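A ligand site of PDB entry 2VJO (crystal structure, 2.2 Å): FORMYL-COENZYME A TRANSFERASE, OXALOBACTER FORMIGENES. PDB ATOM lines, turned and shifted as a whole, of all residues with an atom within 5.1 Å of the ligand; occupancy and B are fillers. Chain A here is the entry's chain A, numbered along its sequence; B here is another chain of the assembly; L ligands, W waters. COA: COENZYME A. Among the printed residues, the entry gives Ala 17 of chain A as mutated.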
ATOM      1  N   HIS A  15      -7.423 -30.323  -0.422  1.00  0.00           N
ATOM      2  CA  HIS A  15      -6.503 -30.845  -1.422  1.00  0.00           C
ATOM      3  C   HIS A  15      -5.061 -30.600  -0.968  1.00  0.00           C
ATOM      4  O   HIS A  15      -4.822 -29.870  -0.008  1.00  0.00           O
ATOM      5  CB  HIS A  15      -6.783 -30.224  -2.809  1.00  0.00           C
ATOM      6  CG  HIS A  15      -6.629 -28.734  -2.863  1.00  0.00           C
ATOM      7  ND1 HIS A  15      -5.779 -28.102  -3.746  1.00  0.00           N
ATOM      8  CD2 HIS A  15      -7.211 -27.748  -2.138  1.00  0.00           C
ATOM      9  CE1 HIS A  15      -5.842 -26.798  -3.560  1.00  0.00           C
ATOM     10  NE2 HIS A  15      -6.697 -26.560  -2.593  1.00  0.00           N
ATOM     11  N   VAL A  16      -4.122 -31.236  -1.665  1.00  0.00           N
ATOM     12  CA  VAL A  16      -2.683 -31.190  -1.350  1.00  0.00           C
ATOM     13  C   VAL A  16      -2.363 -31.944  -0.032  1.00  0.00           C
ATOM     14  O   VAL A  16      -2.739 -33.118   0.098  1.00  0.00           O
ATOM     15  CB  VAL A  16      -2.056 -29.749  -1.447  1.00  0.00           C
ATOM     16  CG1 VAL A  16      -0.538 -29.810  -1.499  1.00  0.00           C
ATOM     17  CG2 VAL A  16      -2.570 -29.025  -2.699  1.00  0.00           C
ATOM     18  N   ALA A  17      -1.709 -31.291   0.926  1.00  0.00           N
ATOM     19  CA  ALA A  17      -1.210 -32.007   2.120  1.00  0.00           C
ATOM     20  C   ALA A  17      -1.740 -31.535   3.482  1.00  0.00           C
ATOM     21  O   ALA A  17      -2.031 -32.371   4.332  1.00  0.00           O
ATOM     22  CB  ALA A  17       0.321 -32.082   2.104  1.00  0.00           C
ATOM     23  N   ALA A  18      -1.847 -30.219   3.692  1.00  0.00           N
ATOM     24  CA  ALA A  18      -2.230 -29.672   5.005  1.00  0.00           C
ATOM     25  C   ALA A  18      -3.630 -30.089   5.443  1.00  0.00           C
ATOM     26  O   ALA A  18      -3.807 -30.723   6.498  1.00  0.00           O
ATOM     27  CB  ALA A  18      -2.088 -28.139   5.034  1.00  0.00           C
ATOM     28  N   ILE A  36     -14.617 -33.938  -1.325  1.00  0.00           N
ATOM     29  CA  ILE A  36     -15.082 -33.291  -2.547  1.00  0.00           C
ATOM     30  C   ILE A  36     -13.874 -32.967  -3.417  1.00  0.00           C
ATOM     31  O   ILE A  36     -12.938 -32.294  -2.975  1.00  0.00           O
ATOM     32  CB  ILE A  36     -15.903 -32.012  -2.254  1.00  0.00           C
ATOM     33  CG1 ILE A  36     -17.213 -32.388  -1.563  1.00  0.00           C
ATOM     34  CG2 ILE A  36     -16.175 -31.196  -3.535  1.00  0.00           C
ATOM     35  CD1 ILE A  36     -17.825 -31.257  -0.802  1.00  0.00           C
ATOM     36  N   GLU A  37     -13.896 -33.473  -4.642  1.00  0.00           N
ATOM     37  CA  GLU A  37     -12.793 -33.303  -5.578  1.00  0.00           C
ATOM     38  C   GLU A  37     -13.281 -32.668  -6.879  1.00  0.00           C
ATOM     39  O   GLU A  37     -14.452 -32.802  -7.242  1.00  0.00           O
ATOM     40  CB  GLU A  37     -12.128 -34.636  -5.880  1.00  0.00           C
ATOM     41  CG  GLU A  37     -11.796 -35.463  -4.648  1.00  0.00           C
ATOM     42  CD  GLU A  37     -10.704 -36.469  -4.902  1.00  0.00           C
ATOM     43  OE1 GLU A  37      -9.656 -36.078  -5.451  1.00  0.00           O
ATOM     44  OE2 GLU A  37     -10.894 -37.645  -4.559  1.00  0.00           O
ATOM     45  N   ARG A  38     -12.366 -31.990  -7.565  1.00  0.00           N
ATOM     46  CA  ARG A  38     -12.622 -31.420  -8.882  1.00  0.00           C
ATOM     47  C   ARG A  38     -12.904 -32.533  -9.902  1.00  0.00           C
ATOM     48  O   ARG A  38     -12.246 -33.581  -9.884  1.00  0.00           O
ATOM     49  CB  ARG A  38     -11.425 -30.586  -9.328  1.00  0.00           C
ATOM     50  CG  ARG A  38     -11.775 -29.174  -9.752  1.00  0.00           C
ATOM     51  CD  ARG A  38     -10.539 -28.382 -10.141  1.00  0.00           C
ATOM     52  NE  ARG A  38     -10.877 -27.000 -10.508  1.00  0.00           N
ATOM     53  CZ  ARG A  38     -10.405 -25.911  -9.904  1.00  0.00           C
ATOM     54  NH1 ARG A  38     -10.776 -24.714 -10.319  1.00  0.00           N
ATOM     55  NH2 ARG A  38      -9.532 -26.017  -8.893  1.00  0.00           N
ATOM     56  N   ARG A  39     -13.879 -32.299 -10.777  1.00  0.00           N
ATOM     57  CA  ARG A  39     -14.238 -33.245 -11.839  1.00  0.00           C
ATOM     58  C   ARG A  39     -13.087 -33.452 -12.804  1.00  0.00           C
ATOM     59  O   ARG A  39     -12.493 -32.471 -13.275  1.00  0.00           O
ATOM     60  CB  ARG A  39     -15.462 -32.752 -12.617  1.00  0.00           C
ATOM     61  CG  ARG A  39     -16.800 -33.314 -12.161  1.00  0.00           C
ATOM     62  CD  ARG A  39     -17.917 -32.905 -13.123  1.00  0.00           C
ATOM     63  NE  ARG A  39     -17.936 -33.714 -14.347  1.00  0.00           N
ATOM     64  CZ  ARG A  39     -17.466 -33.325 -15.529  1.00  0.00           C
ATOM     65  NH1 ARG A  39     -16.928 -32.130 -15.688  1.00  0.00           N
ATOM     66  NH2 ARG A  39     -17.541 -34.151 -16.575  1.00  0.00           N
ATOM     67  N   MET A  44      -4.786 -32.563  -6.735  1.00  0.00           N
ATOM     68  CA  MET A  44      -3.516 -32.463  -7.473  1.00  0.00           C
ATOM     69  C   MET A  44      -2.503 -33.544  -7.123  1.00  0.00           C
ATOM     70  O   MET A  44      -1.670 -33.898  -7.944  1.00  0.00           O
ATOM     71  CB  MET A  44      -2.875 -31.088  -7.249  1.00  0.00           C
ATOM     72  CG  MET A  44      -3.744 -29.871  -7.586  1.00  0.00           C
ATOM     73  SD  MET A  44      -3.393 -28.409  -6.559  1.00  0.00           S
ATOM     74  CE  MET A  44      -4.380 -27.184  -7.416  1.00  0.00           C
ATOM     75  N   LEU A  72     -17.231 -33.137  -8.137  1.00  0.00           N
ATOM     76  CA  LEU A  72     -18.241 -32.086  -8.148  1.00  0.00           C
ATOM     77  C   LEU A  72     -17.713 -30.771  -8.714  1.00  0.00           C
ATOM     78  O   LEU A  72     -16.694 -30.260  -8.242  1.00  0.00           O
ATOM     79  CB  LEU A  72     -18.827 -31.861  -6.741  1.00  0.00           C
ATOM     80  CG  LEU A  72     -20.027 -30.921  -6.562  1.00  0.00           C
ATOM     81  CD1 LEU A  72     -21.315 -31.535  -7.104  1.00  0.00           C
ATOM     82  CD2 LEU A  72     -20.196 -30.535  -5.106  1.00  0.00           C
ATOM     83  N   ASP A  73     -18.401 -30.253  -9.719  1.00  0.00           N
ATOM     84  CA  ASP A  73     -18.205 -28.861 -10.139  1.00  0.00           C
ATOM     85  C   ASP A  73     -19.022 -28.013  -9.175  1.00  0.00           C
ATOM     86  O   ASP A  73     -20.255 -28.103  -9.153  1.00  0.00           O
ATOM     87  CB  ASP A  73     -18.655 -28.636 -11.587  1.00  0.00           C
ATOM     88  CG  ASP A  73     -18.272 -27.249 -12.128  1.00  0.00           C
ATOM     89  OD1 ASP A  73     -17.779 -26.397 -11.352  1.00  0.00           O
ATOM     90  OD2 ASP A  73     -18.459 -27.014 -13.339  1.00  0.00           O
ATOM     91  N   MET A  74     -18.318 -27.194  -8.395  1.00  0.00           N
ATOM     92  CA  MET A  74     -18.957 -26.357  -7.384  1.00  0.00           C
ATOM     93  C   MET A  74     -19.344 -24.973  -7.937  1.00  0.00           C
ATOM     94  O   MET A  74     -20.095 -24.235  -7.295  1.00  0.00           O
ATOM     95  CB  MET A  74     -18.062 -26.221  -6.159  1.00  0.00           C
ATOM     96  CG  MET A  74     -17.904 -27.506  -5.348  1.00  0.00           C
ATOM     97  SD  MET A  74     -16.503 -27.518  -4.198  1.00  0.00           S
ATOM     98  CE  MET A  74     -16.943 -26.198  -3.082  1.00  0.00           C
ATOM     99  N   LYS A  75     -18.848 -24.650  -9.124  1.00  0.00           N
ATOM    100  CA  LYS A  75     -19.207 -23.400  -9.806  1.00  0.00           C
ATOM    101  C   LYS A  75     -20.468 -23.541 -10.677  1.00  0.00           C
ATOM    102  O   LYS A  75     -20.620 -22.859 -11.694  1.00  0.00           O
ATOM    103  CB  LYS A  75     -18.012 -22.839 -10.589  1.00  0.00           C
ATOM    104  CG  LYS A  75     -17.004 -22.120  -9.702  1.00  0.00           C
ATOM    105  CD  LYS A  75     -15.749 -21.656 -10.440  1.00  0.00           C
ATOM    106  CE  LYS A  75     -14.779 -20.968  -9.474  1.00  0.00           C
ATOM    107  NZ  LYS A  75     -13.494 -20.551 -10.102  1.00  0.00           N
ATOM    108  N   ASN A  96      -8.935 -25.954   2.583  1.00  0.00           N
ATOM    109  CA  ASN A  96      -7.664 -25.260   2.443  1.00  0.00           C
ATOM    110  C   ASN A  96      -7.477 -24.732   1.008  1.00  0.00           C
ATOM    111  O   ASN A  96      -6.427 -24.923   0.392  1.00  0.00           O
ATOM    112  CB  ASN A  96      -6.470 -26.122   2.931  1.00  0.00           C
ATOM    113  CG  ASN A  96      -6.195 -27.348   2.055  1.00  0.00           C
ATOM    114  OD1 ASN A  96      -7.070 -28.160   1.798  1.00  0.00           O
ATOM    115  ND2 ASN A  96      -4.945 -27.499   1.633  1.00  0.00           N
ATOM    116  N   PHE A  97      -8.532 -24.094   0.486  1.00  0.00           N
ATOM    117  CA  PHE A  97      -8.445 -23.293  -0.732  1.00  0.00           C
ATOM    118  C   PHE A  97      -7.656 -22.024  -0.424  1.00  0.00           C
ATOM    119  O   PHE A  97      -7.303 -21.751   0.728  1.00  0.00           O
ATOM    120  CB  PHE A  97      -9.825 -22.881  -1.251  1.00  0.00           C
ATOM    121  CG  PHE A  97     -10.698 -24.017  -1.707  1.00  0.00           C
ATOM    122  CD1 PHE A  97     -11.975 -24.180  -1.184  1.00  0.00           C
ATOM    123  CD2 PHE A  97     -10.254 -24.923  -2.678  1.00  0.00           C
ATOM    124  CE1 PHE A  97     -12.808 -25.227  -1.587  1.00  0.00           C
ATOM    125  CE2 PHE A  97     -11.078 -25.972  -3.103  1.00  0.00           C
ATOM    126  CZ  PHE A  97     -12.354 -26.128  -2.559  1.00  0.00           C
ATOM    127  N   GLY A  98      -7.410 -21.226  -1.465  1.00  0.00           N
ATOM    128  CA  GLY A  98      -6.823 -19.904  -1.286  1.00  0.00           C
ATOM    129  C   GLY A  98      -7.770 -18.995  -0.510  1.00  0.00           C
ATOM    130  O   GLY A  98      -8.945 -19.322  -0.356  1.00  0.00           O
ATOM    131  N   PRO A  99      -7.253 -17.855  -0.014  1.00  0.00           N
ATOM    132  CA  PRO A  99      -8.052 -16.903   0.761  1.00  0.00           C
ATOM    133  C   PRO A  99      -9.302 -16.438   0.017  1.00  0.00           C
ATOM    134  O   PRO A  99      -9.233 -16.063  -1.169  1.00  0.00           O
ATOM    135  CB  PRO A  99      -7.072 -15.734   0.996  1.00  0.00           C
ATOM    136  CG  PRO A  99      -5.725 -16.353   0.884  1.00  0.00           C
ATOM    137  CD  PRO A  99      -5.849 -17.413  -0.169  1.00  0.00           C
ATOM    138  N   ALA A 101     -11.791 -17.975  -1.254  1.00  0.00           N
ATOM    139  CA  ALA A 101     -12.304 -18.843  -2.328  1.00  0.00           C
ATOM    140  C   ALA A 101     -13.634 -19.530  -2.027  1.00  0.00           C
ATOM    141  O   ALA A 101     -14.510 -19.588  -2.892  1.00  0.00           O
ATOM    142  CB  ALA A 101     -11.242 -19.880  -2.735  1.00  0.00           C
ATOM    143  N   ARG A 104     -16.356 -16.747  -2.154  1.00  0.00           N
ATOM    144  CA  ARG A 104     -16.775 -16.366  -3.516  1.00  0.00           C
ATOM    145  C   ARG A 104     -17.658 -17.417  -4.177  1.00  0.00           C
ATOM    146  O   ARG A 104     -18.244 -17.176  -5.234  1.00  0.00           O
ATOM    147  CB  ARG A 104     -15.558 -16.070  -4.392  1.00  0.00           C
ATOM    148  CG  ARG A 104     -14.766 -14.835  -3.975  1.00  0.00           C
ATOM    149  CD  ARG A 104     -13.604 -14.575  -4.925  1.00  0.00           C
ATOM    150  NE  ARG A 104     -12.559 -15.581  -4.813  1.00  0.00           N
ATOM    151  CZ  ARG A 104     -11.399 -15.415  -4.172  1.00  0.00           C
ATOM    152  NH1 ARG A 104     -11.134 -14.272  -3.560  1.00  0.00           N
ATOM    153  NH2 ARG A 104     -10.510 -16.396  -4.132  1.00  0.00           N
ATOM    154  N   MET A 105     -17.748 -18.588  -3.548  1.00  0.00           N
ATOM    155  CA  MET A 105     -18.645 -19.651  -3.978  1.00  0.00           C
ATOM    156  C   MET A 105     -20.012 -19.544  -3.303  1.00  0.00           C
ATOM    157  O   MET A 105     -20.870 -20.412  -3.477  1.00  0.00           O
ATOM    158  CB  MET A 105     -18.040 -21.021  -3.676  1.00  0.00           C
ATOM    159  CG  MET A 105     -17.064 -21.513  -4.718  1.00  0.00           C
ATOM    160  SD  MET A 105     -16.504 -23.188  -4.382  1.00  0.00           S
ATOM    161  CE  MET A 105     -15.660 -23.543  -5.913  1.00  0.00           C
ATOM    162  N   VAL A 124      -7.331 -24.066   6.747  1.00  0.00           N
ATOM    163  CA  VAL A 124      -5.893 -23.827   6.682  1.00  0.00           C
ATOM    164  C   VAL A 124      -5.652 -22.710   5.663  1.00  0.00           C
ATOM    165  O   VAL A 124      -6.193 -22.744   4.549  1.00  0.00           O
ATOM    166  CB  VAL A 124      -5.069 -25.091   6.276  1.00  0.00           C
ATOM    167  CG1 VAL A 124      -3.587 -24.737   6.058  1.00  0.00           C
ATOM    168  CG2 VAL A 124      -5.184 -26.187   7.306  1.00  0.00           C
ATOM    169  N   LYS A 125      -4.851 -21.727   6.055  1.00  0.00           N
ATOM    170  CA  LYS A 125      -4.415 -20.638   5.181  1.00  0.00           C
ATOM    171  C   LYS A 125      -2.936 -20.376   5.420  1.00  0.00           C
ATOM    172  O   LYS A 125      -2.394 -20.768   6.448  1.00  0.00           O
ATOM    173  CB  LYS A 125      -5.219 -19.358   5.449  1.00  0.00           C
ATOM    174  CG  LYS A 125      -6.724 -19.460   5.134  1.00  0.00           C
ATOM    175  CD  LYS A 125      -7.023 -19.364   3.631  1.00  0.00           C
ATOM    176  CE  LYS A 125      -8.373 -20.009   3.319  1.00  0.00           C
ATOM    177  NZ  LYS A 125      -8.269 -21.497   3.244  1.00  0.00           N
ATOM    178  N   GLY A 126      -2.287 -19.722   4.456  1.00  0.00           N
ATOM    179  CA  GLY A 126      -0.870 -19.360   4.589  1.00  0.00           C
ATOM    180  C   GLY A 126      -0.606 -18.467   5.782  1.00  0.00           C
ATOM    181  O   GLY A 126       0.260 -18.753   6.616  1.00  0.00           O
ATOM    182  N   LEU A 136      -2.130 -14.016   0.489  1.00  0.00           N
ATOM    183  CA  LEU A 136      -1.117 -14.809  -0.216  1.00  0.00           C
ATOM    184  C   LEU A 136      -1.391 -16.314  -0.238  1.00  0.00           C
ATOM    185  O   LEU A 136      -1.958 -16.880   0.706  1.00  0.00           O
ATOM    186  CB  LEU A 136       0.275 -14.544   0.358  1.00  0.00           C
ATOM    187  CG  LEU A 136       0.866 -13.135   0.349  1.00  0.00           C
ATOM    188  CD1 LEU A 136       2.335 -13.219   0.712  1.00  0.00           C
ATOM    189  CD2 LEU A 136       0.690 -12.422  -0.990  1.00  0.00           C
ATOM    190  N   LYS A 137      -0.994 -16.947  -1.338  1.00  0.00           N
ATOM    191  CA  LYS A 137      -1.054 -18.407  -1.461  1.00  0.00           C
ATOM    192  C   LYS A 137       0.297 -18.966  -1.057  1.00  0.00           C
ATOM    193  O   LYS A 137       1.343 -18.445  -1.464  1.00  0.00           O
ATOM    194  CB  LYS A 137      -1.434 -18.827  -2.875  1.00  0.00           C
ATOM    195  CG  LYS A 137      -2.925 -18.710  -3.176  1.00  0.00           C
ATOM    196  CD  LYS A 137      -3.240 -19.065  -4.630  1.00  0.00           C
ATOM    197  CE  LYS A 137      -4.672 -18.695  -4.996  1.00  0.00           C
ATOM    198  NZ  LYS A 137      -4.887 -18.707  -6.462  1.00  0.00           N
ATOM    199  N   VAL A 138       0.284 -20.012  -0.233  1.00  0.00           N
ATOM    200  CA  VAL A 138       1.530 -20.527   0.339  1.00  0.00           C
ATOM    201  C   VAL A 138       1.673 -22.047   0.229  1.00  0.00           C
ATOM    202  O   VAL A 138       0.741 -22.796   0.525  1.00  0.00           O
ATOM    203  CB  VAL A 138       1.733 -20.044   1.817  1.00  0.00           C
ATOM    204  CG1 VAL A 138       3.003 -20.609   2.407  1.00  0.00           C
ATOM    205  CG2 VAL A 138       1.762 -18.501   1.906  1.00  0.00           C
ATOM    206  N   TYR A 139       2.840 -22.478  -0.240  1.00  0.00           N
ATOM    207  CA  TYR A 139       3.234 -23.888  -0.244  1.00  0.00           C
ATOM    208  C   TYR A 139       4.260 -24.188   0.860  1.00  0.00           C
ATOM    209  O   TYR A 139       4.761 -23.276   1.527  1.00  0.00           O
ATOM    210  CB  TYR A 139       3.771 -24.278  -1.628  1.00  0.00           C
ATOM    211  CG  TYR A 139       2.681 -24.516  -2.660  1.00  0.00           C
ATOM    212  CD1 TYR A 139       1.918 -25.678  -2.627  1.00  0.00           C
ATOM    213  CD2 TYR A 139       2.429 -23.581  -3.660  1.00  0.00           C
ATOM    214  CE1 TYR A 139       0.916 -25.918  -3.558  1.00  0.00           C
ATOM    215  CE2 TYR A 139       1.425 -23.797  -4.607  1.00  0.00           C
ATOM    216  CZ  TYR A 139       0.672 -24.972  -4.548  1.00  0.00           C
ATOM    217  OH  TYR A 139      -0.318 -25.210  -5.470  1.00  0.00           O
ATOM    218  N   GLU A 140       4.593 -25.472   1.023  1.00  0.00           N
ATOM    219  CA  GLU A 140       5.434 -25.961   2.139  1.00  0.00           C
ATOM    220  C   GLU A 140       6.624 -25.075   2.523  1.00  0.00           C
ATOM    221  O   GLU A 140       6.721 -24.609   3.661  1.00  0.00           O
ATOM    222  CB  GLU A 140       5.907 -27.401   1.861  1.00  0.00           C
ATOM    223  CG  GLU A 140       6.856 -27.999   2.914  1.00  0.00           C
ATOM    224  CD  GLU A 140       6.243 -28.064   4.311  1.00  0.00           C
ATOM    225  OE1 GLU A 140       6.857 -27.556   5.271  1.00  0.00           O
ATOM    226  OE2 GLU A 140       5.147 -28.620   4.455  1.00  0.00           O
ATOM    227  N   ASP A 169       2.858 -27.839   5.828  1.00  0.00           N
ATOM    228  CA  ASP A 169       1.613 -28.561   5.500  1.00  0.00           C
ATOM    229  C   ASP A 169       1.110 -29.508   6.598  1.00  0.00           C
ATOM    230  O   ASP A 169       0.118 -29.196   7.256  1.00  0.00           O
ATOM    231  CB  ASP A 169       1.728 -29.211   4.117  1.00  0.00           C
ATOM    232  CG  ASP A 169       1.502 -28.155   3.054  1.00  0.00           C
ATOM    233  OD1 ASP A 169       2.332 -27.284   2.873  1.00  0.00           O
ATOM    234  N   MET A 200      -0.447 -21.354   8.330  1.00  0.00           N
ATOM    235  CA  MET A 200       0.813 -22.112   8.211  1.00  0.00           C
ATOM    236  C   MET A 200       2.004 -21.417   8.871  1.00  0.00           C
ATOM    237  O   MET A 200       2.840 -22.089   9.485  1.00  0.00           O
ATOM    238  CB  MET A 200       1.120 -22.413   6.741  1.00  0.00           C
ATOM    239  CG  MET A 200       0.132 -23.362   6.089  1.00  0.00           C
ATOM    240  SD  MET A 200       0.328 -23.460   4.310  1.00  0.00           S
ATOM    241  CE  MET A 200       1.688 -24.605   4.187  1.00  0.00           C
ATOM    242  N   ASN B 287       0.624 -24.543 -12.656  1.00  0.00           N
ATOM    243  CA  ASN B 287      -0.278 -23.607 -13.344  1.00  0.00           C
ATOM    244  C   ASN B 287       0.254 -22.170 -13.427  1.00  0.00           C
ATOM    245  O   ASN B 287      -0.145 -21.404 -14.297  1.00  0.00           O
ATOM    246  CB  ASN B 287      -1.678 -23.639 -12.731  1.00  0.00           C
ATOM    247  CG  ASN B 287      -1.703 -23.170 -11.269  1.00  0.00           C
ATOM    248  OD1 ASN B 287      -0.703 -23.274 -10.550  1.00  0.00           O
ATOM    249  ND2 ASN B 287      -2.854 -22.683 -10.828  1.00  0.00           N
ATOM    250  N   MET B 288       1.162 -21.841 -12.513  1.00  0.00           N
ATOM    251  CA  MET B 288       1.725 -20.491 -12.398  1.00  0.00           C
ATOM    252  C   MET B 288       2.958 -20.271 -13.298  1.00  0.00           C
ATOM    253  O   MET B 288       3.752 -19.352 -13.068  1.00  0.00           O
ATOM    254  CB  MET B 288       2.098 -20.193 -10.936  1.00  0.00           C
ATOM    255  CG  MET B 288       0.936 -20.245  -9.949  1.00  0.00           C
ATOM    256  SD  MET B 288      -0.117 -18.771  -9.977  1.00  0.00           S
ATOM    257  CE  MET B 288      -1.303 -19.181  -8.687  1.00  0.00           C
HETATM  258  N1A COA L   1     -15.196 -27.045  -8.507  1.00  0.00           N
HETATM  259  C2A COA L   1     -15.150 -25.757  -8.902  1.00  0.00           C
HETATM  260  N3A COA L   1     -14.178 -24.936  -8.481  1.00  0.00           N
HETATM  261  C4A COA L   1     -13.209 -25.392  -7.644  1.00  0.00           C
HETATM  262  C5A COA L   1     -13.238 -26.712  -7.226  1.00  0.00           C
HETATM  263  C6A COA L   1     -14.252 -27.551  -7.680  1.00  0.00           C
HETATM  264  N6A COA L   1     -14.307 -28.820  -7.290  1.00  0.00           N
HETATM  265  N7A COA L   1     -12.173 -26.901  -6.409  1.00  0.00           N
HETATM  266  C8A COA L   1     -11.511 -25.727  -6.321  1.00  0.00           C
HETATM  267  N9A COA L   1     -12.143 -24.811  -7.070  1.00  0.00           N
HETATM  268  C1B COA L   1     -11.753 -23.394  -7.245  1.00  0.00           C
HETATM  269  C2B COA L   1     -11.559 -22.688  -5.902  1.00  0.00           C
HETATM  270  O2B COA L   1     -12.781 -22.272  -5.307  1.00  0.00           O
HETATM  271  C3B COA L   1     -10.719 -21.493  -6.304  1.00  0.00           C
HETATM  272  O3B COA L   1     -11.644 -20.467  -6.652  1.00  0.00           O
HETATM  273  P3B COA L   1     -11.228 -18.988  -7.116  1.00  0.00           P
HETATM  274  O7A COA L   1     -10.053 -18.607  -6.243  1.00  0.00           O
HETATM  275  O8A COA L   1     -10.967 -19.051  -8.606  1.00  0.00           O
HETATM  276  O9A COA L   1     -12.478 -18.165  -6.929  1.00  0.00           O
HETATM  277  C4B COA L   1      -9.937 -21.972  -7.523  1.00  0.00           C
HETATM  278  O4B COA L   1     -10.515 -23.218  -7.933  1.00  0.00           O
HETATM  279  C5B COA L   1      -8.445 -22.151  -7.230  1.00  0.00           C
HETATM  280  O5B COA L   1      -8.271 -22.976  -6.072  1.00  0.00           O
HETATM  281  P1A COA L   1      -7.011 -22.829  -5.084  1.00  0.00           P
HETATM  282  O1A COA L   1      -7.373 -23.586  -3.832  1.00  0.00           O
HETATM  283  O2A COA L   1      -6.656 -21.397  -4.749  1.00  0.00           O
HETATM  284  O3A COA L   1      -5.814 -23.595  -5.854  1.00  0.00           O
HETATM  285  P2A COA L   1      -4.395 -22.970  -6.322  1.00  0.00           P
HETATM  286  O4A COA L   1      -4.575 -21.570  -6.853  1.00  0.00           O
HETATM  287  O5A COA L   1      -3.704 -23.995  -7.183  1.00  0.00           O
HETATM  288  O6A COA L   1      -3.585 -22.836  -4.930  1.00  0.00           O
HETATM  289  CBP COA L   1      -2.926 -23.678  -2.711  1.00  0.00           C
HETATM  290  CCP COA L   1      -3.184 -23.997  -4.185  1.00  0.00           C
HETATM  291  CDP COA L   1      -2.916 -25.028  -1.995  1.00  0.00           C
HETATM  292  CEP COA L   1      -1.556 -23.017  -2.590  1.00  0.00           C
HETATM  293  CAP COA L   1      -4.032 -22.756  -2.153  1.00  0.00           C
HETATM  294  OAP COA L   1      -5.306 -23.384  -2.273  1.00  0.00           O
HETATM  295  C9P COA L   1      -3.789 -22.314  -0.721  1.00  0.00           C
HETATM  296  O9P COA L   1      -3.159 -21.168  -0.462  1.00  0.00           O
HETATM  297  N8P COA L   1      -4.233 -23.077   0.281  1.00  0.00           N
HETATM  298  C7P COA L   1      -4.035 -22.730   1.680  1.00  0.00           C
HETATM  299  C6P COA L   1      -2.634 -23.112   2.198  1.00  0.00           C
HETATM  300  C5P COA L   1      -2.267 -24.535   1.815  1.00  0.00           C
HETATM  301  O5P COA L   1      -3.016 -25.474   2.092  1.00  0.00           O
HETATM  302  N4P COA L   1      -1.096 -24.702   1.192  1.00  0.00           N
HETATM  303  C3P COA L   1      -0.690 -25.960   0.571  1.00  0.00           C
HETATM  304  C2P COA L   1       0.508 -26.633   1.239  1.00  0.00           C
HETATM  305  S1P COA L   1       0.016 -28.122   2.064  1.00  0.00           S
HETATM  306  O   HOH W   1      -3.110 -19.431   1.573  1.00  0.00           O
HETATM  307  O   HOH W   2     -12.069 -29.136  -5.271  1.00  0.00           O
HETATM  308  O   HOH W   3     -14.227 -19.534  -5.558  1.00  0.00           O
HETATM  309  O   HOH W   4      -8.371 -19.451  -4.608  1.00  0.00           O
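S1P of the ligand is covalently linked to CG of Asp 169 (1.8 Å).
The backbone carbonyl oxygen (O) of Val 138 is in hydrogen-bond range of a nitrogen (N4P) of the ligand, at 2.7 Å.
The guanidinium group (NH1) of Arg 38 is in hydrogen-bond range of an oxygen (O4B) of the ligand (2.8 Å).
O of Asn 96 sits at hydrogen-bond distance from N8P of the ligand, at 2.9 Å.
The side-chain amide nitrogen of Asn 96 sits at hydrogen-bond distance from an oxygen (O5P) of the ligand, 2.8 Å away.
The side-chain amino group of Lys 137 lies within salt-bridge range of an oxygen (O4A) of the ligand.
O of Leu 72 sits at hydrogen-bond distance from N6A of the ligand (2.9 Å).
The guanidinium group (NH2) of Arg 104 is in salt-bridge range of an oxygen (O7A) of the ligand (3.1 Å).
N of Gly 98 is in hydrogen-bond range of OAP of the ligand (3.1 Å).
N of Met 74 is in hydrogen-bond range of N1A of the ligand, 3.1 Å away.
A sulfur (S1P) of the ligand sits close to the backbone NH of Ala 18, 3.2 Å away.
A nitrogen (N8P) of the ligand lies within hydrogen-bond range of the backbone carbonyl oxygen of Phe 97, 3.4 Å away.
A ring nitrogen (NE2) of His 15 lies within hydrogen-bond range of an oxygen (O1A) of the ligand, at 3.3 Å.
O8A of the ligand lies within salt-bridge range of NZ of Lys 75 (3.3 Å).
N4P of the ligand lies within hydrogen-bond range of SD of Met 200.
N of Ala 17 sits close to S1P of the ligand, 3.8 Å away.
OE2 of Glu 140 is in hydrogen-bond range of N of Asp 169, at 2.8 Å.
ND2 of Asn 96 lies within hydrogen-bond range of O of His 15, 2.9 Å away.
N of Leu 72 is in hydrogen-bond range of O of Glu 37.
NH2 of Arg 104 is in hydrogen-bond range of O of Pro 99, at 3.2 Å.
The side-chain amino group of Lys 125 sits at hydrogen-bond distance from the backbone carbonyl oxygen of Phe 97, 2.7 Å away.
The side-chain sulfur (SD) of Met 44 lies within hydrogen-bond range of a ring nitrogen (ND1) of His 15 (3.7 Å).
The backbone NH of Lys 75 is in hydrogen-bond range of the side-chain carboxylate of Asp 73.
The backbone carbonyl oxygen (O) of Lys 125 lies within hydrogen-bond range of the backbone NH (N) of Met 200 (2.8 Å).
Val 16 touches the ligand (CG1 to S1P, 3.98 Å).
O of Glu 37 touches N6A of the ligand, at 3.98 Å.
Met 44 touches the ligand.
OD1 of Asp 73 touches C2A of the ligand (3.7 Å).
Ala 101 touches the ligand (CB to O2B, 3.8 Å).
Met 105 touches the ligand (CE to O2B, 3.2 Å).
Val 124 touches the ligand (O to C7P, 3.6 Å).
OH of Tyr 139 touches CCP of the ligand, at 3.4 Å.
Asn 287 of chain B touches the ligand (ND2 to O5A, 3.97 Å).
Hydrophobic or aromatic side chains that line the ligand: His 15, Val 16, Ala 17, Ala 18, Met 44, Met 74, Phe 97, Ala 101, Met 105, Tyr 139 and Met 200.
Water W3 bridges an oxygen (O9A) of the ligand (2.6 Å) and the backbone carbonyl oxygen (O) of Ala 101 (2.7 Å).
Water W1 lies within hydrogen-bond range of O9P of the ligand (2.7 Å), O of Leu 136 (2.9 Å) and N of Gly 126 (3.0 Å).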
